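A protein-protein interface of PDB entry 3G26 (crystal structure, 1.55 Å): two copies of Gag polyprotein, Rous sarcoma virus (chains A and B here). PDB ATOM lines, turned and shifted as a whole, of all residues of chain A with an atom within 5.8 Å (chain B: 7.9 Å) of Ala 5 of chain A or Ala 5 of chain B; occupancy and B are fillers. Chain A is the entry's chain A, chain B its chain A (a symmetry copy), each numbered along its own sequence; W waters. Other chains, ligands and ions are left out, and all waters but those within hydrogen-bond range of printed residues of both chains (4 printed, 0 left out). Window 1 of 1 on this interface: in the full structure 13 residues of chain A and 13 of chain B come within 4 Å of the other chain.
The side-chain carboxylate of Asp 42 of chain B lies within hydrogen-bond range of the indole nitrogen of Trp 4 of chain A (2.8 Å). The backbone NH of Trp 4 of chain A sits at hydrogen-bond distance from the side-chain amide oxygen of Gln 46 of chain B. OE1 of Gln 46 of chain B is in hydrogen-bond range of N of Ala 5 of chain A (2.8 Å). NZ of Lys 47 of chain B sits at hydrogen-bond distance from O of Ala 5 of chain A, 2.8 Å away. NE1 of Trp 4 of chain B sits at hydrogen-bond distance from OD2 of Asp 42 of chain A, 2.8 Å away. The side-chain amide oxygen (OE1) of Gln 46 of chain A lies within hydrogen-bond range of the backbone NH (N) of Trp 4 of chain B (3.4 Å). The backbone NH (N) of Ala 5 of chain B lies within hydrogen-bond range of the side-chain amide oxygen (OE1) of Gln 46 of chain A, 2.8 Å away. NZ of Lys 47 of chain A sits at hydrogen-bond distance from O of Ala 5 of chain B, 2.8 Å away. OD1 of Asp 6 of chain A sits close to O of Gln 46 of chain B (3.3 Å). The backbone carbonyl oxygen of Gln 46 of chain A sits close to the side-chain carboxylate of Asp 6 of chain B.
Water W1 lies within hydrogen-bond range of OD2 of Asp 6 of chain A (2.6 Å) and O of Gln 46 of chain B (2.8 Å). Water W4 lies within hydrogen-bond range of OD2 of Asp 6 of chain B (2.6 Å) and O of Gln 46 of chain A (2.8 Å). Water W3 bridges the side-chain carboxylate of Asp 6 of chain B and the backbone carbonyl oxygen of Gln 46 of chain A. Water W2 bridges the side-chain carboxylate (OD1) of Asp 6 of chain A (3.0 Å) and the backbone carbonyl oxygen (O) of Gln 46 of chain B (3.2 Å).
Of the printed residues of chain B, Pro 3 of chain A touches Gln 46 (3.4 Å). Printed residues of chain B within 4 Å of Trp 4 of chain A: Trp 4, Asp 42 and Gln 46. Ala 5 of chain A touches three residues of chain B. Ala 5 of chain B touches just these residues of chain A: Ala 5 (3.8 Å), Gln 46 (2.8 Å) and Lys 47 (2.8 Å). Ala 25 of chain B touches none of the printed residues of chain A. Cys 43 of chain B touches none of the printed residues of chain A. Of the printed residues of chain A, Gln 46 of chain B touches Pro 3, Trp 4, Ala 5 and Asp 6. The nearest printed residue of chain B that does not touch Asp 6 of chain A is Met 8 of chain B (5.3 Å).
The backbone carbonyl oxygen of Ala 5 of chain A is in hydrogen-bond range of the side-chain amino group of Lys 47 of chain A. The side-chain amino group (NZ) of Lys 47 of chain A sits close to the backbone carbonyl oxygen (O) of Ile 7 of chain A (3.5 Å). The backbone carbonyl oxygen (O) of Ala 5 of chain B lies within hydrogen-bond range of the side-chain amino group (NZ) of Lys 47 of chain B. O of Ile 7 of chain B sits close to NZ of Lys 47 of chain B (3.5 Å).
Among the printed residues, pairs that only touch across the chains: Asp 6 of chain A with Lys 47 of chain B (3.1 Å), Lys 47 of chain A with Asp 6 of chain B (3.1 Å), Pro 3 of chain A with Gln 46 of chain B (3.4 Å), Gln 46 of chain A with Pro 3 of chain B (3.4 Å), Trp 4 of chain A with Trp 4 of chain B (3.6 Å), Ala 5 of chain A with Ala 5 of chain B (3.8 Å) and Lys 47 of chain A with Lys 47 of chain B (3.97 Å).
Hydrophobic or aromatic side chains of chain A within 4 Å of the printed part of chain B: Pro 3, Trp 4 and Ala 5. Along chain A the printed residues that touch a printed residue of chain B span positions 3 to 47. Among the printed residues, no Asp or Glu carboxylate lies within 4 Å of a Lys or Arg side-chain nitrogen of the other chain.
Trp 4 of chain A touches its own counterpart, Trp 4 of chain B. Trp 4 of chain A touches Asp 42 of chain B, and with the chains exchanged Asp 42 of chain A touches Trp 4 of chain B. Ala 5 of chain B touches its own counterpart, Ala 5 of chain A. Asp 6 of chain A touches Gln 46 of chain B, and with the chains exchanged Gln 46 of chain A touches Asp 6 of chain B. Positions printed for both chains: 2, 3, 4, 5, 6, 7, 42, 43, 46 and 47.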
ATOM      1  N   GLY A   2      19.198  11.550   9.274  1.00  0.00           N
ATOM      2  CA  GLY A   2      19.471  11.611   7.825  1.00  0.00           C
ATOM      3  C   GLY A   2      18.217  11.928   7.019  1.00  0.00           C
ATOM      4  O   GLY A   2      17.114  11.623   7.476  1.00  0.00           O
ATOM      5  N   PRO A   3      18.359  12.548   5.813  1.00  0.00           N
ATOM      6  CA  PRO A   3      17.117  12.813   5.125  1.00  0.00           C
ATOM      7  C   PRO A   3      16.611  11.485   4.562  1.00  0.00           C
ATOM      8  O   PRO A   3      17.125  10.933   3.556  1.00  0.00           O
ATOM      9  CB  PRO A   3      17.497  13.845   4.051  1.00  0.00           C
ATOM     10  CG  PRO A   3      19.019  13.786   3.974  1.00  0.00           C
ATOM     11  CD  PRO A   3      19.511  12.755   4.928  1.00  0.00           C
ATOM     12  N   TRP A   4      15.572  10.991   5.222  1.00  0.00           N
ATOM     13  CA  TRP A   4      15.089   9.646   4.939  1.00  0.00           C
ATOM     14  C   TRP A   4      14.621   9.514   3.495  1.00  0.00           C
ATOM     15  O   TRP A   4      14.721   8.439   2.916  1.00  0.00           O
ATOM     16  CB  TRP A   4      13.981   9.231   5.931  1.00  0.00           C
ATOM     17  CG  TRP A   4      12.732  10.081   5.819  1.00  0.00           C
ATOM     18  CD1 TRP A   4      12.432  11.204   6.571  1.00  0.00           C
ATOM     19  CD2 TRP A   4      11.653   9.922   4.884  1.00  0.00           C
ATOM     20  NE1 TRP A   4      11.228  11.742   6.149  1.00  0.00           N
ATOM     21  CE2 TRP A   4      10.726  10.966   5.134  1.00  0.00           C
ATOM     22  CE3 TRP A   4      11.373   9.000   3.855  1.00  0.00           C
ATOM     23  CZ2 TRP A   4       9.529  11.103   4.410  1.00  0.00           C
ATOM     24  CZ3 TRP A   4      10.156   9.136   3.130  1.00  0.00           C
ATOM     25  CH2 TRP A   4       9.255  10.182   3.411  1.00  0.00           C
ATOM     26  N   ALA A   5      14.100  10.595   2.892  1.00  0.00           N
ATOM     27  CA  ALA A   5      13.503  10.444   1.569  1.00  0.00           C
ATOM     28  C   ALA A   5      14.586  10.355   0.482  1.00  0.00           C
ATOM     29  O   ALA A   5      14.282  10.054  -0.675  1.00  0.00           O
ATOM     30  CB  ALA A   5      12.507  11.611   1.282  1.00  0.00           C
ATOM     31  N   ASP A   6      15.837  10.631   0.865  1.00  0.00           N
ATOM     32  CA  ASP A   6      16.980  10.525  -0.053  1.00  0.00           C
ATOM     33  C   ASP A   6      17.614   9.138  -0.027  1.00  0.00           C
ATOM     34  O   ASP A   6      18.513   8.843  -0.827  1.00  0.00           O
ATOM     35  CB  ASP A   6      18.102  11.471   0.391  1.00  0.00           C
ATOM     36  CG  ASP A   6      17.821  12.918   0.122  1.00  0.00           C
ATOM     37  OD1 ASP A   6      16.923  13.262  -0.649  1.00  0.00           O
ATOM     38  OD2 ASP A   6      18.577  13.732   0.697  1.00  0.00           O
ATOM     39  N   ILE A   7      17.207   8.290   0.909  1.00  0.00           N
ATOM     40  CA  ILE A   7      17.920   7.025   1.132  1.00  0.00           C
ATOM     41  C   ILE A   7      17.535   5.948   0.103  1.00  0.00           C
ATOM     42  O   ILE A   7      16.360   5.642  -0.104  1.00  0.00           O
ATOM     43  CB  ILE A   7      17.742   6.544   2.584  1.00  0.00           C
ATOM     44  CG1 ILE A   7      18.437   7.505   3.554  1.00  0.00           C
ATOM     45  CG2 ILE A   7      18.307   5.108   2.782  1.00  0.00           C
ATOM     46  CD1 ILE A   7      18.083   7.229   5.015  1.00  0.00           C
ATOM     47  N   ASP A  42       6.775   1.599   2.196  1.00  0.00           N
ATOM     48  CA  ASP A  42       6.806   2.151   0.846  1.00  0.00           C
ATOM     49  C   ASP A  42       8.238   2.329   0.392  1.00  0.00           C
ATOM     50  O   ASP A  42       8.570   2.047  -0.774  1.00  0.00           O
ATOM     51  CB  ASP A  42       6.078   3.507   0.754  1.00  0.00           C
ATOM     52  CG  ASP A  42       4.593   3.369   0.555  1.00  0.00           C
ATOM     53  OD1 ASP A  42       4.035   2.314   0.894  1.00  0.00           O
ATOM     54  OD2 ASP A  42       3.979   4.309   0.010  1.00  0.00           O
ATOM     55  N   CYS A  43       9.113   2.802   1.285  1.00  0.00           N
ATOM     56  CA  CYS A  43      10.508   2.996   0.888  1.00  0.00           C
ATOM     57  C   CYS A  43      11.220   1.661   0.633  1.00  0.00           C
ATOM     58  O   CYS A  43      12.108   1.581  -0.243  1.00  0.00           O
ATOM     59  CB  CYS A  43      11.296   3.807   1.919  1.00  0.00           C
ATOM     60  SG  CYS A  43      10.784   5.557   1.944  1.00  0.00           S
ATOM     61  N   GLN A  46      10.212   0.761  -2.877  1.00  0.00           N
ATOM     62  CA  GLN A  46      10.561   1.694  -3.955  1.00  0.00           C
ATOM     63  C   GLN A  46      12.046   2.007  -4.041  1.00  0.00           C
ATOM     64  O   GLN A  46      12.546   2.381  -5.107  1.00  0.00           O
ATOM     65  CB  GLN A  46       9.809   3.022  -3.756  1.00  0.00           C
ATOM     66  CG  GLN A  46       8.297   2.853  -3.852  1.00  0.00           C
ATOM     67  CD  GLN A  46       7.570   4.148  -3.575  1.00  0.00           C
ATOM     68  OE1 GLN A  46       8.095   5.216  -3.861  1.00  0.00           O
ATOM     69  NE2 GLN A  46       6.365   4.065  -3.038  1.00  0.00           N
ATOM     70  N   LYS A  47      12.745   1.855  -2.920  1.00  0.00           N
ATOM     71  CA  LYS A  47      14.106   2.402  -2.823  1.00  0.00           C
ATOM     72  C   LYS A  47      15.195   1.368  -2.639  1.00  0.00           C
ATOM     73  O   LYS A  47      16.395   1.713  -2.586  1.00  0.00           O
ATOM     74  CB  LYS A  47      14.157   3.436  -1.673  1.00  0.00           C
ATOM     75  CG  LYS A  47      13.083   4.537  -1.777  1.00  0.00           C
ATOM     76  CD  LYS A  47      13.175   5.408  -3.077  1.00  0.00           C
ATOM     77  CE  LYS A  47      14.377   6.397  -2.981  1.00  0.00           C
ATOM     78  NZ  LYS A  47      14.131   7.506  -2.055  1.00  0.00           N
ATOM     79  N   GLY B   2       2.742   7.049  -9.557  1.00  0.00           N
ATOM     80  CA  GLY B   2       4.215   7.042  -9.647  1.00  0.00           C
ATOM     81  C   GLY B   2       4.868   6.705  -8.311  1.00  0.00           C
ATOM     82  O   GLY B   2       4.266   6.958  -7.266  1.00  0.00           O
ATOM     83  N   PRO B   3       6.102   6.127  -8.318  1.00  0.00           N
ATOM     84  CA  PRO B   3       6.638   5.841  -7.009  1.00  0.00           C
ATOM     85  C   PRO B   3       7.088   7.167  -6.395  1.00  0.00           C
ATOM     86  O   PRO B   3       8.130   7.767  -6.760  1.00  0.00           O
ATOM     87  CB  PRO B   3       7.787   4.856  -7.280  1.00  0.00           C
ATOM     88  CG  PRO B   3       8.051   4.969  -8.777  1.00  0.00           C
ATOM     89  CD  PRO B   3       7.132   5.987  -9.354  1.00  0.00           C
ATOM     90  N   TRP B   4       6.287   7.606  -5.432  1.00  0.00           N
ATOM     91  CA  TRP B   4       6.460   8.941  -4.878  1.00  0.00           C
ATOM     92  C   TRP B   4       7.829   9.100  -4.228  1.00  0.00           C
ATOM     93  O   TRP B   4       8.379  10.195  -4.221  1.00  0.00           O
ATOM     94  CB  TRP B   4       5.324   9.288  -3.892  1.00  0.00           C
ATOM     95  CG  TRP B   4       5.308   8.398  -2.666  1.00  0.00           C
ATOM     96  CD1 TRP B   4       4.563   7.244  -2.496  1.00  0.00           C
ATOM     97  CD2 TRP B   4       6.094   8.549  -1.472  1.00  0.00           C
ATOM     98  NE1 TRP B   4       4.848   6.678  -1.265  1.00  0.00           N
ATOM     99  CE2 TRP B   4       5.766   7.467  -0.616  1.00  0.00           C
ATOM    100  CE3 TRP B   4       7.048   9.491  -1.036  1.00  0.00           C
ATOM    101  CZ2 TRP B   4       6.338   7.311   0.658  1.00  0.00           C
ATOM    102  CZ3 TRP B   4       7.619   9.336   0.257  1.00  0.00           C
ATOM    103  CH2 TRP B   4       7.264   8.252   1.084  1.00  0.00           C
ATOM    104  N   ALA B   5       8.398   8.020  -3.668  1.00  0.00           N
ATOM    105  CA  ALA B   5       9.630   8.191  -2.904  1.00  0.00           C
ATOM    106  C   ALA B   5      10.841   8.350  -3.838  1.00  0.00           C
ATOM    107  O   ALA B   5      11.940   8.675  -3.381  1.00  0.00           O
ATOM    108  CB  ALA B   5       9.830   7.000  -1.915  1.00  0.00           C
ATOM    109  N   ASP B   6      10.627   8.106  -5.135  1.00  0.00           N
ATOM    110  CA  ASP B   6      11.676   8.279  -6.148  1.00  0.00           C
ATOM    111  C   ASP B   6      11.683   9.685  -6.738  1.00  0.00           C
ATOM    112  O   ASP B   6      12.579  10.034  -7.520  1.00  0.00           O
ATOM    113  CB  ASP B   6      11.409   7.359  -7.346  1.00  0.00           C
ATOM    114  CG  ASP B   6      11.691   5.911  -7.077  1.00  0.00           C
ATOM    115  OD1 ASP B   6      12.355   5.560  -6.101  1.00  0.00           O
ATOM    116  OD2 ASP B   6      11.244   5.107  -7.924  1.00  0.00           O
ATOM    117  N   ILE B   7      10.675  10.490  -6.428  1.00  0.00           N
ATOM    118  CA  ILE B   7      10.499  11.771  -7.125  1.00  0.00           C
ATOM    119  C   ILE B   7      11.435  12.865  -6.580  1.00  0.00           C
ATOM    120  O   ILE B   7      11.483  13.137  -5.379  1.00  0.00           O
ATOM    121  CB  ILE B   7       9.021  12.202  -7.117  1.00  0.00           C
ATOM    122  CG1 ILE B   7       8.179  11.236  -7.958  1.00  0.00           C
ATOM    123  CG2 ILE B   7       8.846  13.650  -7.659  1.00  0.00           C
ATOM    124  CD1 ILE B   7       6.677  11.456  -7.783  1.00  0.00           C
ATOM    125  N   MET B   8      12.187  13.476  -7.496  1.00  0.00           N
ATOM    126  CA  MET B   8      13.042  14.602  -7.108  1.00  0.00           C
ATOM    127  C   MET B   8      12.918  15.663  -8.207  1.00  0.00           C
ATOM    128  O   MET B   8      12.654  15.354  -9.351  1.00  0.00           O
ATOM    129  CB  MET B   8      14.488  14.171  -6.872  1.00  0.00           C
ATOM    130  CG  MET B   8      15.131  13.594  -8.050  1.00  0.00           C
ATOM    131  SD  MET B   8      16.807  13.064  -7.637  1.00  0.00           S
ATOM    132  CE  MET B   8      16.727  12.562  -5.940  1.00  0.00           C
ATOM    133  N   LEU B  22       4.938  15.217  -7.395  1.00  0.00           N
ATOM    134  CA  LEU B  22       5.070  14.587  -6.080  1.00  0.00           C
ATOM    135  C   LEU B  22       3.700  14.372  -5.441  1.00  0.00           C
ATOM    136  O   LEU B  22       3.383  13.254  -4.975  1.00  0.00           O
ATOM    137  CB  LEU B  22       5.949  15.453  -5.167  1.00  0.00           C
ATOM    138  CG  LEU B  22       6.005  15.015  -3.701  1.00  0.00           C
ATOM    139  CD1 LEU B  22       6.796  13.715  -3.514  1.00  0.00           C
ATOM    140  CD2 LEU B  22       6.629  16.126  -2.893  1.00  0.00           C
ATOM    141  N   ALA B  25       1.599  11.674  -7.046  1.00  0.00           N
ATOM    142  CA  ALA B  25       2.105  10.346  -6.702  1.00  0.00           C
ATOM    143  C   ALA B  25       1.730   9.984  -5.269  1.00  0.00           C
ATOM    144  O   ALA B  25       1.334   8.840  -5.002  1.00  0.00           O
ATOM    145  CB  ALA B  25       3.630  10.263  -6.919  1.00  0.00           C
ATOM    146  N   VAL B  26       1.860  10.926  -4.333  1.00  0.00           N
ATOM    147  CA  VAL B  26       1.469  10.647  -2.955  1.00  0.00           C
ATOM    148  C   VAL B  26      -0.044  10.349  -2.848  1.00  0.00           C
ATOM    149  O   VAL B  26      -0.451   9.399  -2.186  1.00  0.00           O
ATOM    150  CB  VAL B  26       1.904  11.780  -1.985  1.00  0.00           C
ATOM    151  CG1 VAL B  26       1.274  11.604  -0.582  1.00  0.00           C
ATOM    152  CG2 VAL B  26       3.444  11.845  -1.907  1.00  0.00           C
ATOM    153  N   SER B  29      -0.835   6.883  -3.762  1.00  0.00           N
ATOM    154  CA  SER B  29      -0.048   5.890  -2.998  1.00  0.00           C
ATOM    155  C   SER B  29      -0.945   5.094  -2.047  1.00  0.00           C
ATOM    156  O   SER B  29      -2.130   5.421  -1.870  1.00  0.00           O
ATOM    157  CB  SER B  29       1.065   6.578  -2.194  1.00  0.00           C
ATOM    158  OG  SER B  29       0.549   7.143  -1.011  1.00  0.00           O
ATOM    159  N   VAL B  39       4.274  13.703   4.711  1.00  0.00           N
ATOM    160  CA  VAL B  39       5.197  13.106   3.740  1.00  0.00           C
ATOM    161  C   VAL B  39       5.474  14.102   2.599  1.00  0.00           C
ATOM    162  O   VAL B  39       6.630  14.307   2.198  1.00  0.00           O
ATOM    163  CB  VAL B  39       4.646  11.777   3.206  1.00  0.00           C
ATOM    164  CG1 VAL B  39       5.320  11.334   1.905  1.00  0.00           C
ATOM    165  CG2 VAL B  39       4.765  10.712   4.303  1.00  0.00           C
ATOM    166  N   ASP B  42       7.863  16.777   3.956  1.00  0.00           N
ATOM    167  CA  ASP B  42       9.225  16.267   4.079  1.00  0.00           C
ATOM    168  C   ASP B  42       9.860  16.152   2.710  1.00  0.00           C
ATOM    169  O   ASP B  42      11.049  16.481   2.537  1.00  0.00           O
ATOM    170  CB  ASP B  42       9.271  14.890   4.770  1.00  0.00           C
ATOM    171  CG  ASP B  42       9.278  14.984   6.273  1.00  0.00           C
ATOM    172  OD1 ASP B  42       8.835  16.008   6.815  1.00  0.00           O
ATOM    173  OD2 ASP B  42       9.773  14.040   6.922  1.00  0.00           O
ATOM    174  N   CYS B  43       9.101  15.683   1.716  1.00  0.00           N
ATOM    175  CA  CYS B  43       9.675  15.549   0.377  1.00  0.00           C
ATOM    176  C   CYS B  43       9.971  16.915  -0.256  1.00  0.00           C
ATOM    177  O   CYS B  43      10.949  17.051  -1.024  1.00  0.00           O
ATOM    178  CB  CYS B  43       8.780  14.735  -0.559  1.00  0.00           C
ATOM    179  SG  CYS B  43       8.751  12.968  -0.108  1.00  0.00           S
ATOM    180  N   PHE B  44       9.151  17.933   0.027  1.00  0.00           N
ATOM    181  CA  PHE B  44       9.501  19.274  -0.466  1.00  0.00           C
ATOM    182  C   PHE B  44      10.829  19.736   0.126  1.00  0.00           C
ATOM    183  O   PHE B  44      11.654  20.355  -0.556  1.00  0.00           O
ATOM    184  CB  PHE B  44       8.476  20.313  -0.018  1.00  0.00           C
ATOM    185  CG  PHE B  44       7.152  20.292  -0.748  1.00  0.00           C
ATOM    186  CD1 PHE B  44       6.901  19.477  -1.851  1.00  0.00           C
ATOM    187  CD2 PHE B  44       6.159  21.190  -0.340  1.00  0.00           C
ATOM    188  CE1 PHE B  44       5.649  19.533  -2.524  1.00  0.00           C
ATOM    189  CE2 PHE B  44       4.934  21.252  -0.994  1.00  0.00           C
ATOM    190  CZ  PHE B  44       4.648  20.439  -2.053  1.00  0.00           C
ATOM    191  N   ARG B  45      10.998  19.476   1.422  1.00  0.00           N
ATOM    192  CA  ARG B  45      12.205  19.916   2.129  1.00  0.00           C
ATOM    193  C   ARG B  45      13.447  19.157   1.642  1.00  0.00           C
ATOM    194  O   ARG B  45      14.545  19.732   1.627  1.00  0.00           O
ATOM    195  CB  ARG B  45      12.045  19.696   3.646  1.00  0.00           C
ATOM    196  CG  ARG B  45      11.012  20.579   4.313  1.00  0.00           C
ATOM    197  CD  ARG B  45      10.931  20.367   5.835  1.00  0.00           C
ATOM    198  NE  ARG B  45       9.772  21.074   6.393  1.00  0.00           N
ATOM    199  CZ  ARG B  45       9.663  22.394   6.590  1.00  0.00           C
ATOM    200  NH1 ARG B  45      10.653  23.231   6.285  1.00  0.00           N
ATOM    201  NH2 ARG B  45       8.541  22.878   7.119  1.00  0.00           N
ATOM    202  N   GLN B  46      13.294  17.886   1.214  1.00  0.00           N
ATOM    203  CA  GLN B  46      14.439  16.999   0.975  1.00  0.00           C
ATOM    204  C   GLN B  46      14.721  16.738  -0.496  1.00  0.00           C
ATOM    205  O   GLN B  46      15.854  16.415  -0.868  1.00  0.00           O
ATOM    206  CB  GLN B  46      14.193  15.640   1.656  1.00  0.00           C
ATOM    207  CG  GLN B  46      14.093  15.760   3.172  1.00  0.00           C
ATOM    208  CD  GLN B  46      13.773  14.433   3.819  1.00  0.00           C
ATOM    209  OE1 GLN B  46      14.159  13.393   3.302  1.00  0.00           O
ATOM    210  NE2 GLN B  46      13.086  14.458   4.948  1.00  0.00           N
ATOM    211  N   LYS B  47      13.692  16.880  -1.326  1.00  0.00           N
ATOM    212  CA  LYS B  47      13.785  16.378  -2.704  1.00  0.00           C
ATOM    213  C   LYS B  47      13.704  17.443  -3.775  1.00  0.00           C
ATOM    214  O   LYS B  47      13.814  17.137  -4.982  1.00  0.00           O
ATOM    215  CB  LYS B  47      12.687  15.312  -2.932  1.00  0.00           C
ATOM    216  CG  LYS B  47      12.693  14.178  -1.886  1.00  0.00           C
ATOM    217  CD  LYS B  47      14.024  13.351  -1.840  1.00  0.00           C
ATOM    218  CE  LYS B  47      14.112  12.401  -3.073  1.00  0.00           C
ATOM    219  NZ  LYS B  47      13.202  11.257  -2.980  1.00  0.00           N
HETATM  220  O   HOH W   1      18.179  16.320   0.639  1.00  0.00           O
HETATM  221  O   HOH W   2      16.986  14.666  -3.277  1.00  0.00           O
HETATM  222  O   HOH W   3      15.016   4.240  -5.873  1.00  0.00           O
HETATM  223  O   HOH W   4      11.339   2.510  -7.600  1.00  0.00           O
